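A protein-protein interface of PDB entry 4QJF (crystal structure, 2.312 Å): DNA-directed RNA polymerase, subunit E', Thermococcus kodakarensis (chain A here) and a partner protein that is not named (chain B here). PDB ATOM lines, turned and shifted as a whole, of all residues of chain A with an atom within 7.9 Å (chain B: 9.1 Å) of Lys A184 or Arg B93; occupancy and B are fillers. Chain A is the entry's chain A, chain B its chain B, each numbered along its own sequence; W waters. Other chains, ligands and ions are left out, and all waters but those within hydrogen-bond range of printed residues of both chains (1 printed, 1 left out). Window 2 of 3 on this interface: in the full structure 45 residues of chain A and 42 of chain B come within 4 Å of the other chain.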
ATOM      1  N   VAL A  84       3.619  -0.638 -16.420  1.00  0.00           N
ATOM      2  CA  VAL A  84       3.457   0.431 -17.380  1.00  0.00           C
ATOM      3  C   VAL A  84       2.153   0.202 -18.124  1.00  0.00           C
ATOM      4  O   VAL A  84       1.878  -0.911 -18.569  1.00  0.00           O
ATOM      5  CB  VAL A  84       4.655   0.510 -18.358  1.00  0.00           C
ATOM      6  CG1 VAL A  84       4.375   1.510 -19.501  1.00  0.00           C
ATOM      7  CG2 VAL A  84       5.940   0.871 -17.591  1.00  0.00           C
ATOM      8  N   ARG A 145       2.559   4.911 -15.315  1.00  0.00           N
ATOM      9  CA  ARG A 145       2.970   3.761 -14.527  1.00  0.00           C
ATOM     10  C   ARG A 145       2.080   3.664 -13.293  1.00  0.00           C
ATOM     11  O   ARG A 145       1.883   4.660 -12.589  1.00  0.00           O
ATOM     12  CB  ARG A 145       4.460   3.858 -14.120  1.00  0.00           C
ATOM     13  CG  ARG A 145       4.938   2.686 -13.231  1.00  0.00           C
ATOM     14  CD  ARG A 145       6.360   2.868 -12.661  1.00  0.00           C
ATOM     15  NE  ARG A 145       7.381   3.037 -13.699  1.00  0.00           N
ATOM     16  CZ  ARG A 145       7.832   2.056 -14.476  1.00  0.00           C
ATOM     17  NH1 ARG A 145       7.352   0.820 -14.341  1.00  0.00           N
ATOM     18  NH2 ARG A 145       8.758   2.303 -15.393  1.00  0.00           N
ATOM     19  N   PRO A 168      10.481   9.831 -16.716  1.00  0.00           N
ATOM     20  CA  PRO A 168      10.981   9.791 -18.097  1.00  0.00           C
ATOM     21  C   PRO A 168      10.334   8.700 -18.959  1.00  0.00           C
ATOM     22  O   PRO A 168      10.351   7.527 -18.594  1.00  0.00           O
ATOM     23  CB  PRO A 168      12.482   9.530 -17.906  1.00  0.00           C
ATOM     24  CG  PRO A 168      12.782  10.182 -16.607  1.00  0.00           C
ATOM     25  CD  PRO A 168      11.585   9.856 -15.740  1.00  0.00           C
ATOM     26  N   GLY A 169       9.771   9.102 -20.095  1.00  0.00           N
ATOM     27  CA  GLY A 169       9.113   8.180 -21.004  1.00  0.00           C
ATOM     28  C   GLY A 169       7.622   8.009 -20.725  1.00  0.00           C
ATOM     29  O   GLY A 169       6.963   7.168 -21.336  1.00  0.00           O
ATOM     30  N   LYS A 178       7.886  14.708 -28.173  1.00  0.00           N
ATOM     31  CA  LYS A 178       8.750  15.877 -28.070  1.00  0.00           C
ATOM     32  C   LYS A 178       9.831  15.720 -26.997  1.00  0.00           C
ATOM     33  O   LYS A 178      10.818  16.442 -27.027  1.00  0.00           O
ATOM     34  CB  LYS A 178       7.924  17.139 -27.813  1.00  0.00           C
ATOM     35  CG  LYS A 178       7.345  17.724 -29.095  1.00  0.00           C
ATOM     36  CD  LYS A 178       6.526  18.982 -28.847  1.00  0.00           C
ATOM     37  CE  LYS A 178       5.039  18.682 -28.920  1.00  0.00           C
ATOM     38  NZ  LYS A 178       4.719  17.868 -30.132  1.00  0.00           N
ATOM     39  N   GLU A 179       9.666  14.780 -26.066  1.00  0.00           N
ATOM     40  CA  GLU A 179      10.732  14.490 -25.104  1.00  0.00           C
ATOM     41  C   GLU A 179      11.883  13.806 -25.812  1.00  0.00           C
ATOM     42  O   GLU A 179      13.031  13.911 -25.387  1.00  0.00           O
ATOM     43  CB  GLU A 179      10.280  13.573 -23.953  1.00  0.00           C
ATOM     44  CG  GLU A 179       9.061  13.980 -23.137  1.00  0.00           C
ATOM     45  CD  GLU A 179       9.293  15.152 -22.203  1.00  0.00           C
ATOM     46  OE1 GLU A 179      10.451  15.611 -22.072  1.00  0.00           O
ATOM     47  OE2 GLU A 179       8.301  15.608 -21.591  1.00  0.00           O
ATOM     48  N   LYS A 180      11.567  13.078 -26.879  1.00  0.00           N
ATOM     49  CA  LYS A 180      12.514  12.131 -27.456  1.00  0.00           C
ATOM     50  C   LYS A 180      13.655  12.798 -28.212  1.00  0.00           C
ATOM     51  O   LYS A 180      14.101  13.882 -27.849  1.00  0.00           O
ATOM     52  CB  LYS A 180      11.784  11.150 -28.366  1.00  0.00           C
ATOM     53  CG  LYS A 180      11.554   9.813 -27.708  1.00  0.00           C
ATOM     54  CD  LYS A 180      10.356   9.098 -28.291  1.00  0.00           C
ATOM     55  CE  LYS A 180       9.990   7.902 -27.439  1.00  0.00           C
ATOM     56  NZ  LYS A 180       9.065   6.987 -28.163  1.00  0.00           N
ATOM     57  N   LYS A 181      14.129  12.149 -29.269  1.00  0.00           N
ATOM     58  CA  LYS A 181      15.348  12.597 -29.940  1.00  0.00           C
ATOM     59  C   LYS A 181      15.253  13.987 -30.602  1.00  0.00           C
ATOM     60  O   LYS A 181      16.148  14.377 -31.362  1.00  0.00           O
ATOM     61  CB  LYS A 181      15.786  11.548 -30.967  1.00  0.00           C
ATOM     62  CG  LYS A 181      16.257  10.239 -30.331  1.00  0.00           C
ATOM     63  CD  LYS A 181      17.140   9.432 -31.266  1.00  0.00           C
ATOM     64  CE  LYS A 181      17.687   8.209 -30.558  1.00  0.00           C
ATOM     65  NZ  LYS A 181      18.491   7.373 -31.482  1.00  0.00           N
ATOM     66  N   LYS A 182      14.176  14.720 -30.305  1.00  0.00           N
ATOM     67  CA  LYS A 182      14.122  16.153 -30.559  1.00  0.00           C
ATOM     68  C   LYS A 182      14.688  16.836 -29.341  1.00  0.00           C
ATOM     69  O   LYS A 182      14.970  18.029 -29.364  1.00  0.00           O
ATOM     70  CB  LYS A 182      12.702  16.645 -30.817  1.00  0.00           C
ATOM     71  CG  LYS A 182      12.501  17.356 -32.149  1.00  0.00           C
ATOM     72  CD  LYS A 182      12.286  16.365 -33.271  1.00  0.00           C
ATOM     73  CE  LYS A 182      12.609  16.982 -34.620  1.00  0.00           C
ATOM     74  NZ  LYS A 182      14.071  17.204 -34.798  1.00  0.00           N
ATOM     75  N   ALA A 183      14.822  16.070 -28.262  1.00  0.00           N
ATOM     76  CA  ALA A 183      15.620  16.494 -27.118  1.00  0.00           C
ATOM     77  C   ALA A 183      16.891  15.627 -27.048  1.00  0.00           C
ATOM     78  O   ALA A 183      17.530  15.562 -25.999  1.00  0.00           O
ATOM     79  CB  ALA A 183      14.821  16.400 -25.821  1.00  0.00           C
ATOM     80  N   LYS A 184      17.217  14.936 -28.149  1.00  0.00           N
ATOM     81  CA  LYS A 184      18.552  14.380 -28.393  1.00  0.00           C
ATOM     82  C   LYS A 184      19.056  14.926 -29.731  1.00  0.00           C
ATOM     83  O   LYS A 184      19.869  14.293 -30.412  1.00  0.00           O
ATOM     84  CB  LYS A 184      18.542  12.853 -28.404  1.00  0.00           C
ATOM     85  CG  LYS A 184      18.315  12.209 -27.041  1.00  0.00           C
ATOM     86  CD  LYS A 184      18.462  10.695 -27.106  1.00  0.00           C
ATOM     87  CE  LYS A 184      18.224  10.048 -25.750  1.00  0.00           C
ATOM     88  NZ  LYS A 184      18.239   8.559 -25.839  1.00  0.00           N
ATOM     89  N   GLU A 185      18.553  16.104 -30.096  1.00  0.00           N
ATOM     90  CA  GLU A 185      19.089  16.866 -31.214  1.00  0.00           C
ATOM     91  C   GLU A 185      20.478  17.363 -30.830  1.00  0.00           C
ATOM     92  O   GLU A 185      20.664  18.545 -30.527  1.00  0.00           O
ATOM     93  CB  GLU A 185      18.170  18.037 -31.571  1.00  0.00           C
ATOM     94  CG  GLU A 185      16.937  17.657 -32.383  1.00  0.00           C
ATOM     95  CD  GLU A 185      16.100  18.863 -32.786  1.00  0.00           C
ATOM     96  OE1 GLU A 185      16.051  19.843 -32.014  1.00  0.00           O
ATOM     97  OE2 GLU A 185      15.492  18.833 -33.878  1.00  0.00           O
ATOM     98  N   GLU A 186      21.442  16.445 -30.838  1.00  0.00           N
ATOM     99  CA  GLU A 186      22.789  16.718 -30.352  1.00  0.00           C
ATOM    100  C   GLU A 186      23.816  16.669 -31.481  1.00  0.00           C
ATOM    101  O   GLU A 186      24.182  17.703 -32.046  1.00  0.00           O
ATOM    102  CB  GLU A 186      23.156  15.719 -29.248  1.00  0.00           C
ATOM    103  CG  GLU A 186      22.141  15.669 -28.109  1.00  0.00           C
ATOM    104  CD  GLU A 186      22.555  14.736 -26.987  1.00  0.00           C
ATOM    105  OE1 GLU A 186      23.184  13.699 -27.279  1.00  0.00           O
ATOM    106  OE2 GLU A 186      22.254  15.045 -25.814  1.00  0.00           O
ATOM    107  N   LEU B  81       5.842  -5.750 -23.791  1.00  0.00           N
ATOM    108  CA  LEU B  81       6.589  -5.254 -24.949  1.00  0.00           C
ATOM    109  C   LEU B  81       5.696  -5.201 -26.182  1.00  0.00           C
ATOM    110  O   LEU B  81       5.746  -4.240 -26.941  1.00  0.00           O
ATOM    111  CB  LEU B  81       7.825  -6.127 -25.229  1.00  0.00           C
ATOM    112  CG  LEU B  81       9.029  -6.010 -24.290  1.00  0.00           C
ATOM    113  CD1 LEU B  81      10.075  -7.070 -24.603  1.00  0.00           C
ATOM    114  CD2 LEU B  81       9.648  -4.623 -24.356  1.00  0.00           C
ATOM    115  N   PRO B  86       7.468  -0.453 -27.994  1.00  0.00           N
ATOM    116  CA  PRO B  86       8.490   0.582 -27.793  1.00  0.00           C
ATOM    117  C   PRO B  86       9.251   0.939 -29.069  1.00  0.00           C
ATOM    118  O   PRO B  86       9.609   0.036 -29.828  1.00  0.00           O
ATOM    119  CB  PRO B  86       9.430  -0.056 -26.758  1.00  0.00           C
ATOM    120  CG  PRO B  86       9.210  -1.505 -26.900  1.00  0.00           C
ATOM    121  CD  PRO B  86       7.744  -1.636 -27.169  1.00  0.00           C
ATOM    122  N   GLU B  87       9.494   2.232 -29.290  1.00  0.00           N
ATOM    123  CA  GLU B  87      10.141   2.708 -30.519  1.00  0.00           C
ATOM    124  C   GLU B  87      11.648   2.916 -30.380  1.00  0.00           C
ATOM    125  O   GLU B  87      12.394   2.682 -31.331  1.00  0.00           O
ATOM    126  CB  GLU B  87       9.503   4.021 -30.987  1.00  0.00           C
ATOM    127  CG  GLU B  87       8.080   3.899 -31.519  1.00  0.00           C
ATOM    128  CD  GLU B  87       7.438   5.260 -31.769  1.00  0.00           C
ATOM    129  OE1 GLU B  87       8.021   6.284 -31.340  1.00  0.00           O
ATOM    130  OE2 GLU B  87       6.354   5.311 -32.391  1.00  0.00           O
ATOM    131  N   ASP B  88      12.098   3.373 -29.211  1.00  0.00           N
ATOM    132  CA  ASP B  88      13.526   3.616 -28.992  1.00  0.00           C
ATOM    133  C   ASP B  88      13.992   3.266 -27.578  1.00  0.00           C
ATOM    134  O   ASP B  88      13.283   2.605 -26.820  1.00  0.00           O
ATOM    135  CB  ASP B  88      13.875   5.073 -29.302  1.00  0.00           C
ATOM    136  CG  ASP B  88      12.922   6.049 -28.651  1.00  0.00           C
ATOM    137  OD1 ASP B  88      12.609   7.083 -29.281  1.00  0.00           O
ATOM    138  OD2 ASP B  88      12.484   5.783 -27.512  1.00  0.00           O
ATOM    139  N   TYR B  89      15.193   3.723 -27.235  1.00  0.00           N
ATOM    140  CA  TYR B  89      15.848   3.338 -25.984  1.00  0.00           C
ATOM    141  C   TYR B  89      15.103   3.838 -24.756  1.00  0.00           C
ATOM    142  O   TYR B  89      15.110   3.191 -23.701  1.00  0.00           O
ATOM    143  CB  TYR B  89      17.296   3.853 -25.948  1.00  0.00           C
ATOM    144  CG  TYR B  89      18.077   3.323 -24.768  1.00  0.00           C
ATOM    145  CD1 TYR B  89      18.144   1.959 -24.520  1.00  0.00           C
ATOM    146  CD2 TYR B  89      18.746   4.176 -23.901  1.00  0.00           C
ATOM    147  CE1 TYR B  89      18.852   1.456 -23.443  1.00  0.00           C
ATOM    148  CE2 TYR B  89      19.463   3.680 -22.815  1.00  0.00           C
ATOM    149  CZ  TYR B  89      19.510   2.316 -22.593  1.00  0.00           C
ATOM    150  OH  TYR B  89      20.210   1.797 -21.523  1.00  0.00           O
ATOM    151  N   LEU B  90      14.466   4.994 -24.901  1.00  0.00           N
ATOM    152  CA  LEU B  90      13.718   5.593 -23.809  1.00  0.00           C
ATOM    153  C   LEU B  90      12.515   4.714 -23.491  1.00  0.00           C
ATOM    154  O   LEU B  90      12.173   4.523 -22.326  1.00  0.00           O
ATOM    155  CB  LEU B  90      13.277   7.022 -24.163  1.00  0.00           C
ATOM    156  CG  LEU B  90      13.191   8.077 -23.043  1.00  0.00           C
ATOM    157  CD1 LEU B  90      12.040   9.052 -23.281  1.00  0.00           C
ATOM    158  CD2 LEU B  90      13.090   7.473 -21.654  1.00  0.00           C
ATOM    159  N   ASP B  91      11.879   4.166 -24.525  1.00  0.00           N
ATOM    160  CA  ASP B  91      10.678   3.362 -24.304  1.00  0.00           C
ATOM    161  C   ASP B  91      11.027   2.054 -23.588  1.00  0.00           C
ATOM    162  O   ASP B  91      10.296   1.621 -22.677  1.00  0.00           O
ATOM    163  CB  ASP B  91       9.952   3.069 -25.621  1.00  0.00           C
ATOM    164  CG  ASP B  91       9.362   4.321 -26.270  1.00  0.00           C
ATOM    165  OD1 ASP B  91       9.099   5.321 -25.560  1.00  0.00           O
ATOM    166  OD2 ASP B  91       9.152   4.287 -27.502  1.00  0.00           O
ATOM    167  N   ILE B  92      12.146   1.451 -24.007  1.00  0.00           N
ATOM    168  CA  ILE B  92      12.699   0.247 -23.392  1.00  0.00           C
ATOM    169  C   ILE B  92      13.080   0.521 -21.923  1.00  0.00           C
ATOM    170  O   ILE B  92      12.857  -0.309 -21.051  1.00  0.00           O
ATOM    171  CB  ILE B  92      13.946  -0.274 -24.179  1.00  0.00           C
ATOM    172  CG1 ILE B  92      13.578  -0.611 -25.634  1.00  0.00           C
ATOM    173  CG2 ILE B  92      14.565  -1.502 -23.495  1.00  0.00           C
ATOM    174  CD1 ILE B  92      12.731  -1.861 -25.778  1.00  0.00           C
ATOM    175  N   ARG B  93      13.642   1.696 -21.660  1.00  0.00           N
ATOM    176  CA  ARG B  93      14.054   2.052 -20.311  1.00  0.00           C
ATOM    177  C   ARG B  93      12.862   2.025 -19.363  1.00  0.00           C
ATOM    178  O   ARG B  93      12.915   1.396 -18.305  1.00  0.00           O
ATOM    179  CB  ARG B  93      14.704   3.440 -20.283  1.00  0.00           C
ATOM    180  CG  ARG B  93      16.217   3.447 -20.197  1.00  0.00           C
ATOM    181  CD  ARG B  93      16.712   4.819 -19.769  1.00  0.00           C
ATOM    182  NE  ARG B  93      16.431   5.828 -20.787  1.00  0.00           N
ATOM    183  CZ  ARG B  93      17.368   6.550 -21.396  1.00  0.00           C
ATOM    184  NH1 ARG B  93      18.641   6.381 -21.067  1.00  0.00           N
ATOM    185  NH2 ARG B  93      17.034   7.443 -22.324  1.00  0.00           N
ATOM    186  N   VAL B  94      11.777   2.693 -19.743  1.00  0.00           N
ATOM    187  CA  VAL B  94      10.658   2.796 -18.818  1.00  0.00           C
ATOM    188  C   VAL B  94       9.959   1.438 -18.628  1.00  0.00           C
ATOM    189  O   VAL B  94       9.476   1.129 -17.539  1.00  0.00           O
ATOM    190  CB  VAL B  94       9.649   3.878 -19.257  1.00  0.00           C
ATOM    191  CG1 VAL B  94       8.707   3.381 -20.370  1.00  0.00           C
ATOM    192  CG2 VAL B  94       8.851   4.323 -18.058  1.00  0.00           C
ATOM    193  N   ILE B  95       9.934   0.622 -19.674  1.00  0.00           N
ATOM    194  CA  ILE B  95       9.372  -0.709 -19.569  1.00  0.00           C
ATOM    195  C   ILE B  95      10.174  -1.562 -18.564  1.00  0.00           C
ATOM    196  O   ILE B  95       9.587  -2.270 -17.734  1.00  0.00           O
ATOM    197  CB  ILE B  95       9.323  -1.401 -20.957  1.00  0.00           C
ATOM    198  CG1 ILE B  95       8.233  -0.765 -21.830  1.00  0.00           C
ATOM    199  CG2 ILE B  95       9.070  -2.898 -20.811  1.00  0.00           C
ATOM    200  CD1 ILE B  95       8.218  -1.252 -23.272  1.00  0.00           C
ATOM    201  N   PHE B  96      11.506  -1.463 -18.612  1.00  0.00           N
ATOM    202  CA  PHE B  96      12.363  -2.295 -17.768  1.00  0.00           C
ATOM    203  C   PHE B  96      12.832  -1.643 -16.451  1.00  0.00           C
ATOM    204  O   PHE B  96      13.514  -2.294 -15.651  1.00  0.00           O
ATOM    205  CB  PHE B  96      13.595  -2.754 -18.570  1.00  0.00           C
ATOM    206  CG  PHE B  96      13.288  -3.810 -19.605  1.00  0.00           C
ATOM    207  CD1 PHE B  96      12.930  -3.453 -20.894  1.00  0.00           C
ATOM    208  CD2 PHE B  96      13.346  -5.161 -19.276  1.00  0.00           C
ATOM    209  CE1 PHE B  96      12.641  -4.418 -21.846  1.00  0.00           C
ATOM    210  CE2 PHE B  96      13.054  -6.138 -20.220  1.00  0.00           C
ATOM    211  CZ  PHE B  96      12.701  -5.770 -21.512  1.00  0.00           C
ATOM    212  N   ALA B  97      12.454  -0.386 -16.212  1.00  0.00           N
ATOM    213  CA  ALA B  97      12.969   0.370 -15.065  1.00  0.00           C
ATOM    214  C   ALA B  97      12.721  -0.302 -13.708  1.00  0.00           C
ATOM    215  O   ALA B  97      13.533  -0.184 -12.791  1.00  0.00           O
ATOM    216  CB  ALA B  97      12.374   1.780 -15.056  1.00  0.00           C
ATOM    217  N   LYS B  98      11.593  -0.995 -13.589  1.00  0.00           N
ATOM    218  CA  LYS B  98      11.196  -1.613 -12.333  1.00  0.00           C
ATOM    219  C   LYS B  98      11.369  -3.122 -12.392  1.00  0.00           C
ATOM    220  O   LYS B  98      10.878  -3.851 -11.526  1.00  0.00           O
ATOM    221  CB  LYS B  98       9.742  -1.264 -11.997  1.00  0.00           C
ATOM    222  CG  LYS B  98       9.550   0.187 -11.622  1.00  0.00           C
ATOM    223  CD  LYS B  98      10.601   0.584 -10.583  1.00  0.00           C
ATOM    224  CE  LYS B  98      10.434   2.027 -10.155  1.00  0.00           C
ATOM    225  NZ  LYS B  98      11.389   2.388  -9.067  1.00  0.00           N
ATOM    226  N   GLU B  99      12.067  -3.587 -13.422  1.00  0.00           N
ATOM    227  CA  GLU B  99      12.264  -5.014 -13.601  1.00  0.00           C
ATOM    228  C   GLU B  99      13.587  -5.489 -13.026  1.00  0.00           C
ATOM    229  O   GLU B  99      14.441  -4.695 -12.631  1.00  0.00           O
ATOM    230  CB  GLU B  99      12.182  -5.394 -15.081  1.00  0.00           C
ATOM    231  CG  GLU B  99      10.822  -5.168 -15.699  1.00  0.00           C
ATOM    232  CD  GLU B  99       9.753  -6.103 -15.158  1.00  0.00           C
ATOM    233  OE1 GLU B  99      10.087  -7.030 -14.391  1.00  0.00           O
ATOM    234  OE2 GLU B  99       8.569  -5.908 -15.512  1.00  0.00           O
ATOM    235  N   TYR B 101      16.202  -6.882 -14.532  1.00  0.00           N
ATOM    236  CA  TYR B 101      17.419  -6.548 -15.269  1.00  0.00           C
ATOM    237  C   TYR B 101      17.149  -5.474 -16.315  1.00  0.00           C
ATOM    238  O   TYR B 101      16.112  -5.475 -16.960  1.00  0.00           O
ATOM    239  CB  TYR B 101      18.020  -7.811 -15.926  1.00  0.00           C
ATOM    240  CG  TYR B 101      19.157  -7.536 -16.903  1.00  0.00           C
ATOM    241  CD1 TYR B 101      18.929  -7.498 -18.273  1.00  0.00           C
ATOM    242  CD2 TYR B 101      20.458  -7.308 -16.452  1.00  0.00           C
ATOM    243  CE1 TYR B 101      19.960  -7.232 -19.168  1.00  0.00           C
ATOM    244  CE2 TYR B 101      21.508  -7.048 -17.345  1.00  0.00           C
ATOM    245  CZ  TYR B 101      21.250  -7.013 -18.698  1.00  0.00           C
ATOM    246  OH  TYR B 101      22.269  -6.758 -19.594  1.00  0.00           O
ATOM    247  N   MET B 102      18.106  -4.562 -16.468  1.00  0.00           N
ATOM    248  CA  MET B 102      17.990  -3.416 -17.354  1.00  0.00           C
ATOM    249  C   MET B 102      18.817  -3.586 -18.629  1.00  0.00           C
ATOM    250  O   MET B 102      20.047  -3.612 -18.582  1.00  0.00           O
ATOM    251  CB  MET B 102      18.441  -2.148 -16.632  1.00  0.00           C
ATOM    252  CG  MET B 102      18.507  -0.943 -17.552  1.00  0.00           C
ATOM    253  SD  MET B 102      16.832  -0.482 -18.095  1.00  0.00           S
ATOM    254  CE  MET B 102      17.167   0.088 -19.752  1.00  0.00           C
ATOM    255  N   PRO B 103      18.143  -3.692 -19.778  1.00  0.00           N
ATOM    256  CA  PRO B 103      18.820  -3.871 -21.065  1.00  0.00           C
ATOM    257  C   PRO B 103      19.805  -2.745 -21.384  1.00  0.00           C
ATOM    258  O   PRO B 103      19.433  -1.577 -21.362  1.00  0.00           O
ATOM    259  CB  PRO B 103      17.661  -3.877 -22.071  1.00  0.00           C
ATOM    260  CG  PRO B 103      16.465  -4.277 -21.275  1.00  0.00           C
ATOM    261  CD  PRO B 103      16.681  -3.660 -19.924  1.00  0.00           C
ATOM    262  N   THR B 104      21.049  -3.111 -21.667  1.00  0.00           N
ATOM    263  CA  THR B 104      22.046  -2.198 -22.200  1.00  0.00           C
ATOM    264  C   THR B 104      21.568  -1.639 -23.530  1.00  0.00           C
ATOM    265  O   THR B 104      20.670  -2.219 -24.153  1.00  0.00           O
ATOM    266  CB  THR B 104      23.402  -2.902 -22.440  1.00  0.00           C
ATOM    267  OG1 THR B 104      23.306  -3.718 -23.616  1.00  0.00           O
ATOM    268  CG2 THR B 104      23.831  -3.744 -21.228  1.00  0.00           C
ATOM    269  N   PRO B 105      22.176  -0.522 -23.986  1.00  0.00           N
ATOM    270  CA  PRO B 105      21.801   0.054 -25.281  1.00  0.00           C
ATOM    271  C   PRO B 105      21.726  -0.977 -26.398  1.00  0.00           C
ATOM    272  O   PRO B 105      20.810  -0.941 -27.213  1.00  0.00           O
ATOM    273  CB  PRO B 105      22.923   1.065 -25.549  1.00  0.00           C
ATOM    274  CG  PRO B 105      23.340   1.517 -24.202  1.00  0.00           C
ATOM    275  CD  PRO B 105      23.138   0.339 -23.265  1.00  0.00           C
ATOM    276  N   ALA B 108      18.901  -3.499 -26.090  1.00  0.00           N
ATOM    277  CA  ALA B 108      17.735  -2.656 -26.362  1.00  0.00           C
ATOM    278  C   ALA B 108      17.478  -2.514 -27.863  1.00  0.00           C
ATOM    279  O   ALA B 108      16.343  -2.643 -28.325  1.00  0.00           O
ATOM    280  CB  ALA B 108      17.911  -1.284 -25.729  1.00  0.00           C
ATOM    281  N   ILE B 111      15.932  -5.767 -29.369  1.00  0.00           N
ATOM    282  CA  ILE B 111      14.495  -5.806 -29.149  1.00  0.00           C
ATOM    283  C   ILE B 111      13.743  -4.894 -30.117  1.00  0.00           C
ATOM    284  O   ILE B 111      12.811  -5.323 -30.808  1.00  0.00           O
ATOM    285  CB  ILE B 111      14.165  -5.407 -27.711  1.00  0.00           C
ATOM    286  CG1 ILE B 111      14.790  -6.422 -26.744  1.00  0.00           C
ATOM    287  CG2 ILE B 111      12.678  -5.316 -27.525  1.00  0.00           C
ATOM    288  CD1 ILE B 111      14.747  -5.991 -25.306  1.00  0.00           C
ATOM    289  N   ILE B 112      14.166  -3.639 -30.167  1.00  0.00           N
ATOM    290  CA  ILE B 112      13.548  -2.650 -31.040  1.00  0.00           C
ATOM    291  C   ILE B 112      13.547  -3.104 -32.507  1.00  0.00           C
ATOM    292  O   ILE B 112      12.556  -2.924 -33.213  1.00  0.00           O
ATOM    293  CB  ILE B 112      14.256  -1.297 -30.904  1.00  0.00           C
ATOM    294  CG1 ILE B 112      14.009  -0.738 -29.507  1.00  0.00           C
ATOM    295  CG2 ILE B 112      13.752  -0.319 -31.938  1.00  0.00           C
ATOM    296  CD1 ILE B 112      14.961   0.347 -29.126  1.00  0.00           C
HETATM  297  O   HOH W   1       6.888   5.309 -28.476  1.00  0.00           O
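Hydrophobic or aromatic side chains of chain B that line the printed part of chain A: Leu B90, Val B94 and Ala B97.
Hydrophobic or aromatic side chains of chain A within 4 Å of the printed part of chain B: Val A84.
Water W1 lies within hydrogen-bond range of OD2 of Asp B91 (2.7 Å), NZ of Lys A180 (2.8 Å) and OE1 of Glu B87 (3.2 Å).
N of Glu B87 sits at hydrogen-bond distance from OD2 of Asp B91 (2.7 Å).
The backbone NH (N) of Asp B91 is in hydrogen-bond range of the side-chain carboxylate (OD2) of Asp B88 (3.5 Å).
The side-chain carboxylate (OD2) of Asp B88 lies close to the backbone NH (N) of Leu B90, at 3.4 Å.
Val B94 touches Val A84 (O to CG2, 3.5 Å).
NH2 of Arg A145 touches CB of Ala B97, 3.7 Å away.
Lys B98 touches Arg A145 (CG to NH1, 3.6 Å).
Pro A168 touches Val B94 (O to CG2, 3.6 Å).
CD1 of Leu B90 touches CA of Gly A169, at 3.8 Å.
NZ of Lys A184 touches NH2 of Arg B93, 3.9 Å away.
The side-chain amino group of Lys A180 is in salt-bridge range of the side-chain carboxylate of Asp B88, at 3.7 Å.
NH2 of Arg A145 is in hydrogen-bond range of O of Val B94 (2.5 Å).
OD2 of Asp B91 lies within salt-bridge range of NZ of Lys A180 (2.8 Å).
NZ of Lys A180 is in salt-bridge range of OE1 of Glu B87, 3.4 Å away.
Lys A184 touches one residue of chain B.
Arg B93 touches just one residue of chain A: Lys A184.
No residue of chain B comes within 4 Å of Ala A183.
Printed residues of chain B within 4 Å of Arg A145: Val B94, Ala B97 and Lys B98.
Of the printed residues of chain B, Val A84 touches Val B94 (3.5 Å).
Printed residues of chain A within 4 Å of Glu B87: Lys A180 (3.4 Å).
Leu B81 touches none of the printed residues of chain A.
Ile B95 touches none of the printed residues of chain A.
The nearest residue of chain B that does not touch Lys A184 is Tyr B89 (4.8 Å).
The nearest printed residue of chain B that does not touch Arg A145 is Ile B95 (4.7 Å).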
